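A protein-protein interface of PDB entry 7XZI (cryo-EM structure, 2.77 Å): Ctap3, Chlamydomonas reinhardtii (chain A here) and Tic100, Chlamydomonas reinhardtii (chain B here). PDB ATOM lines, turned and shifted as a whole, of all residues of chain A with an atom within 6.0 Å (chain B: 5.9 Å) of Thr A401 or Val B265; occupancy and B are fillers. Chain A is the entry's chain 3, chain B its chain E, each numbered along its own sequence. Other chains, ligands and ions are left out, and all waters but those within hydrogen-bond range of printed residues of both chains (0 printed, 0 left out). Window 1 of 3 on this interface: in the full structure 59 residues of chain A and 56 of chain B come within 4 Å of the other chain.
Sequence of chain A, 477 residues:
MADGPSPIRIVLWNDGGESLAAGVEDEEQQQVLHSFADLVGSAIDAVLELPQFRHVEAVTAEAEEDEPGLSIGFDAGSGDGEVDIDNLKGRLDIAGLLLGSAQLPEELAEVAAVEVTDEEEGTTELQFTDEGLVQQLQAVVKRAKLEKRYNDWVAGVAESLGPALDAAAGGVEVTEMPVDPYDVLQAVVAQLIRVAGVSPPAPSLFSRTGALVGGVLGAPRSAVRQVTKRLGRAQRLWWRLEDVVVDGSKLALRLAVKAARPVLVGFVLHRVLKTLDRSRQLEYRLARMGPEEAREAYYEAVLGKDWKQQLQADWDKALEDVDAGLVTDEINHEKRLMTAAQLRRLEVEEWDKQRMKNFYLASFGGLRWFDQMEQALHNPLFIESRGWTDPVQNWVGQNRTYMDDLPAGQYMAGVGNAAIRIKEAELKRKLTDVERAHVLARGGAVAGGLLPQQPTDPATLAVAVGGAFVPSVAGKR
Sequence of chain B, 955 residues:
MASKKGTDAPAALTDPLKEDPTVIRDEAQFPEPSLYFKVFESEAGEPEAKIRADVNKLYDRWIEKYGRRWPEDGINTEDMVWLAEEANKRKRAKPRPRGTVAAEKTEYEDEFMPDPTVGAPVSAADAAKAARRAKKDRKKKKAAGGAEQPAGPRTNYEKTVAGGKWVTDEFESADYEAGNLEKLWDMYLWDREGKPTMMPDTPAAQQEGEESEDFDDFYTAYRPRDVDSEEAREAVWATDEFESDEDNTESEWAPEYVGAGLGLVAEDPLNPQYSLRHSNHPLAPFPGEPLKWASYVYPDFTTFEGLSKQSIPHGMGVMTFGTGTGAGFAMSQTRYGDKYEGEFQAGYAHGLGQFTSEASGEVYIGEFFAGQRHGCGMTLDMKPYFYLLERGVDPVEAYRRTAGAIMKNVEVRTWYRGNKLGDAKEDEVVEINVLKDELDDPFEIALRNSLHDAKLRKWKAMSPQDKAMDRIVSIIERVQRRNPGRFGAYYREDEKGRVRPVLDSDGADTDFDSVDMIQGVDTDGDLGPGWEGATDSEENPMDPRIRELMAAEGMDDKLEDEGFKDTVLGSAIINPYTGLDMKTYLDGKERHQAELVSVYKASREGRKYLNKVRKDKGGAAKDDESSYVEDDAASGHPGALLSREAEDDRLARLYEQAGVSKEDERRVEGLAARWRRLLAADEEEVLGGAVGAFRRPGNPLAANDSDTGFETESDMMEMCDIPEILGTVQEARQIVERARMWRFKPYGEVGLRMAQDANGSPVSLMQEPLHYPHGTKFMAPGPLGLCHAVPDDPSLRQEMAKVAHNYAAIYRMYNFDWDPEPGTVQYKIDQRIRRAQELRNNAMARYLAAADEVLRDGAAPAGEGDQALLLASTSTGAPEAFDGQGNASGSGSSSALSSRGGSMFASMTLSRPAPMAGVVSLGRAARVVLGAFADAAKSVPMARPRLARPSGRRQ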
ATOM      1  N   GLN A 398       0.865  18.601  21.288  1.00  0.00           N
ATOM      2  CA  GLN A 398       0.246  19.907  21.428  1.00  0.00           C
ATOM      3  C   GLN A 398       0.377  20.390  22.871  1.00  0.00           C
ATOM      4  O   GLN A 398       0.938  19.708  23.732  1.00  0.00           O
ATOM      5  CB  GLN A 398      -1.214  19.848  20.974  1.00  0.00           C
ATOM      6  CG  GLN A 398      -2.082  18.918  21.797  1.00  0.00           C
ATOM      7  CD  GLN A 398      -3.524  18.917  21.336  1.00  0.00           C
ATOM      8  OE1 GLN A 398      -3.861  19.513  20.313  1.00  0.00           O
ATOM      9  NE2 GLN A 398      -4.386  18.248  22.091  1.00  0.00           N
ATOM     10  N   ASN A 399      -0.148  21.581  23.143  1.00  0.00           N
ATOM     11  CA  ASN A 399      -0.043  22.207  24.450  1.00  0.00           C
ATOM     12  C   ASN A 399      -1.426  22.380  25.061  1.00  0.00           C
ATOM     13  O   ASN A 399      -2.436  22.464  24.357  1.00  0.00           O
ATOM     14  CB  ASN A 399       0.665  23.566  24.360  1.00  0.00           C
ATOM     15  CG  ASN A 399      -0.049  24.534  23.439  1.00  0.00           C
ATOM     16  OD1 ASN A 399       0.094  24.469  22.218  1.00  0.00           O
ATOM     17  ND2 ASN A 399      -0.819  25.445  24.020  1.00  0.00           N
ATOM     18  N   ARG A 400      -1.458  22.434  26.390  1.00  0.00           N
ATOM     19  CA  ARG A 400      -2.710  22.588  27.121  1.00  0.00           C
ATOM     20  C   ARG A 400      -3.214  24.016  26.967  1.00  0.00           C
ATOM     21  O   ARG A 400      -2.523  24.969  27.339  1.00  0.00           O
ATOM     22  CB  ARG A 400      -2.507  22.235  28.592  1.00  0.00           C
ATOM     23  CG  ARG A 400      -3.733  22.438  29.461  1.00  0.00           C
ATOM     24  CD  ARG A 400      -3.510  21.869  30.851  1.00  0.00           C
ATOM     25  NE  ARG A 400      -2.332  22.439  31.490  1.00  0.00           N
ATOM     26  CZ  ARG A 400      -1.876  22.072  32.683  1.00  0.00           C
ATOM     27  NH1 ARG A 400      -2.477  21.133  33.394  1.00  0.00           N
ATOM     28  NH2 ARG A 400      -0.789  22.662  33.171  1.00  0.00           N
ATOM     29  N   THR A 401      -4.419  24.164  26.423  1.00  0.00           N
ATOM     30  CA  THR A 401      -5.000  25.467  26.133  1.00  0.00           C
ATOM     31  C   THR A 401      -6.231  25.678  26.999  1.00  0.00           C
ATOM     32  O   THR A 401      -7.096  24.801  27.081  1.00  0.00           O
ATOM     33  CB  THR A 401      -5.374  25.589  24.653  1.00  0.00           C
ATOM     34  OG1 THR A 401      -6.395  24.636  24.339  1.00  0.00           O
ATOM     35  CG2 THR A 401      -4.163  25.326  23.776  1.00  0.00           C
ATOM     36  N   TYR A 402      -6.305  26.843  27.642  1.00  0.00           N
ATOM     37  CA  TYR A 402      -7.464  27.218  28.449  1.00  0.00           C
ATOM     38  C   TYR A 402      -8.348  28.123  27.598  1.00  0.00           C
ATOM     39  O   TYR A 402      -8.346  29.347  27.724  1.00  0.00           O
ATOM     40  CB  TYR A 402      -7.024  27.898  29.741  1.00  0.00           C
ATOM     41  CG  TYR A 402      -5.957  27.143  30.497  1.00  0.00           C
ATOM     42  CD1 TYR A 402      -6.292  26.132  31.385  1.00  0.00           C
ATOM     43  CD2 TYR A 402      -4.613  27.443  30.323  1.00  0.00           C
ATOM     44  CE1 TYR A 402      -5.319  25.441  32.078  1.00  0.00           C
ATOM     45  CE2 TYR A 402      -3.634  26.758  31.011  1.00  0.00           C
ATOM     46  CZ  TYR A 402      -3.992  25.757  31.887  1.00  0.00           C
ATOM     47  OH  TYR A 402      -3.018  25.072  32.574  1.00  0.00           O
ATOM     48  N   MET A 403      -9.123  27.496  26.713  1.00  0.00           N
ATOM     49  CA  MET A 403      -9.953  28.237  25.775  1.00  0.00           C
ATOM     50  C   MET A 403     -11.158  28.893  26.434  1.00  0.00           C
ATOM     51  O   MET A 403     -11.753  29.796  25.837  1.00  0.00           O
ATOM     52  CB  MET A 403     -10.426  27.310  24.652  1.00  0.00           C
ATOM     53  CG  MET A 403     -10.718  28.020  23.340  1.00  0.00           C
ATOM     54  SD  MET A 403      -9.226  28.676  22.566  1.00  0.00           S
ATOM     55  CE  MET A 403      -8.255  27.182  22.383  1.00  0.00           C
ATOM     56  N   ASP A 404     -11.532  28.467  27.640  1.00  0.00           N
ATOM     57  CA  ASP A 404     -12.665  29.056  28.341  1.00  0.00           C
ATOM     58  C   ASP A 404     -12.292  30.300  29.135  1.00  0.00           C
ATOM     59  O   ASP A 404     -13.187  31.058  29.525  1.00  0.00           O
ATOM     60  CB  ASP A 404     -13.297  28.027  29.284  1.00  0.00           C
ATOM     61  CG  ASP A 404     -13.677  26.740  28.574  1.00  0.00           C
ATOM     62  OD1 ASP A 404     -12.765  26.009  28.134  1.00  0.00           O
ATOM     63  OD2 ASP A 404     -14.889  26.458  28.459  1.00  0.00           O
ATOM     64  N   PRO A 455      -9.860  25.075  15.498  1.00  0.00           N
ATOM     65  CA  PRO A 455      -8.657  25.917  15.362  1.00  0.00           C
ATOM     66  C   PRO A 455      -7.762  25.537  14.195  1.00  0.00           C
ATOM     67  O   PRO A 455      -7.105  26.411  13.618  1.00  0.00           O
ATOM     68  CB  PRO A 455      -7.946  25.721  16.708  1.00  0.00           C
ATOM     69  CG  PRO A 455      -9.035  25.362  17.656  1.00  0.00           C
ATOM     70  CD  PRO A 455     -10.003  24.538  16.862  1.00  0.00           C
ATOM     71  N   GLY B 263       5.199  24.974  16.550  1.00  0.00           N
ATOM     72  CA  GLY B 263       3.926  24.305  16.379  1.00  0.00           C
ATOM     73  C   GLY B 263       3.122  24.236  17.660  1.00  0.00           C
ATOM     74  O   GLY B 263       3.349  23.359  18.499  1.00  0.00           O
ATOM     75  N   LEU B 264       2.176  25.158  17.821  1.00  0.00           N
ATOM     76  CA  LEU B 264       1.340  25.229  19.009  1.00  0.00           C
ATOM     77  C   LEU B 264      -0.059  25.673  18.610  1.00  0.00           C
ATOM     78  O   LEU B 264      -0.247  26.339  17.590  1.00  0.00           O
ATOM     79  CB  LEU B 264       1.913  26.199  20.054  1.00  0.00           C
ATOM     80  CG  LEU B 264       3.282  25.890  20.665  1.00  0.00           C
ATOM     81  CD1 LEU B 264       3.763  27.052  21.518  1.00  0.00           C
ATOM     82  CD2 LEU B 264       3.231  24.611  21.485  1.00  0.00           C
ATOM     83  N   VAL B 265      -1.040  25.292  19.425  1.00  0.00           N
ATOM     84  CA  VAL B 265      -2.405  25.755  19.218  1.00  0.00           C
ATOM     85  C   VAL B 265      -2.547  27.155  19.797  1.00  0.00           C
ATOM     86  O   VAL B 265      -2.280  27.385  20.985  1.00  0.00           O
ATOM     87  CB  VAL B 265      -3.407  24.780  19.852  1.00  0.00           C
ATOM     88  CG1 VAL B 265      -4.829  25.283  19.670  1.00  0.00           C
ATOM     89  CG2 VAL B 265      -3.246  23.391  19.251  1.00  0.00           C
ATOM     90  N   ALA B 266      -2.967  28.101  18.962  1.00  0.00           N
ATOM     91  CA  ALA B 266      -3.051  29.504  19.355  1.00  0.00           C
ATOM     92  C   ALA B 266      -4.416  29.763  19.983  1.00  0.00           C
ATOM     93  O   ALA B 266      -5.445  29.675  19.307  1.00  0.00           O
ATOM     94  CB  ALA B 266      -2.816  30.414  18.154  1.00  0.00           C
ATOM     95  N   GLU B 267      -4.422  30.081  21.280  1.00  0.00           N
ATOM     96  CA  GLU B 267      -5.668  30.448  21.945  1.00  0.00           C
ATOM     97  C   GLU B 267      -6.232  31.736  21.362  1.00  0.00           C
ATOM     98  O   GLU B 267      -7.443  31.856  21.142  1.00  0.00           O
ATOM     99  CB  GLU B 267      -5.435  30.589  23.449  1.00  0.00           C
ATOM    100  CG  GLU B 267      -4.657  29.438  24.061  1.00  0.00           C
ATOM    101  CD  GLU B 267      -4.339  29.668  25.524  1.00  0.00           C
ATOM    102  OE1 GLU B 267      -5.100  30.399  26.191  1.00  0.00           O
ATOM    103  OE2 GLU B 267      -3.323  29.122  26.004  1.00  0.00           O
ATOM    104  N   SER B 275       0.378  32.257  23.831  1.00  0.00           N
ATOM    105  CA  SER B 275       0.425  30.859  24.242  1.00  0.00           C
ATOM    106  C   SER B 275       1.740  30.471  24.905  1.00  0.00           C
ATOM    107  O   SER B 275       1.860  29.331  25.369  1.00  0.00           O
ATOM    108  CB  SER B 275       0.167  29.953  23.036  1.00  0.00           C
ATOM    109  OG  SER B 275      -1.120  30.187  22.495  1.00  0.00           O
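OD1 of Asn A399 lies within hydrogen-bond range of N of Val B265 (3.1 Å).
OG of Ser B275 sits at hydrogen-bond distance from O of Val B265, at 3.4 Å. OH of Tyr A402 lies within hydrogen-bond range of NE of Arg A400 (2.9 Å).
OD1 of Asn A399 touches CD2 of Leu B264, at 3.2 Å. Thr A401 touches Val B265 (CG2 to O, 3.9 Å). CG of Glu B267 touches CB of Thr A401 (3.96 Å). Tyr A402 touches Glu B267. Glu B267 touches Met A403 (O to SD, 3.9 Å).
Thr A401 touches just these residues of chain B: Val B265 (3.9 Å) and Glu B267 (3.96 Å). Printed residues of chain B within 4 Å of Tyr A402: Glu B267. Of the printed residues of chain B, Met A403 touches Glu B267. Val B265 touches two residues of chain A. The nearest residue of chain B that does not touch Thr A401 is Ala B266 (5.7 Å). The nearest printed residue of chain A that does not touch Glu B267 is Arg A400 (4.4 Å).
Of the 6 printed residues of chain B, 3 touch a printed residue of chain A. Printed residues of chain B that touch a printed residue of chain A: Leu B264, Val B265 and Glu B267. Of the 8 printed residues of chain A, 4 touch a printed residue of chain B. Along chain A the printed residues that touch a printed residue of chain B span positions 399 to 403.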
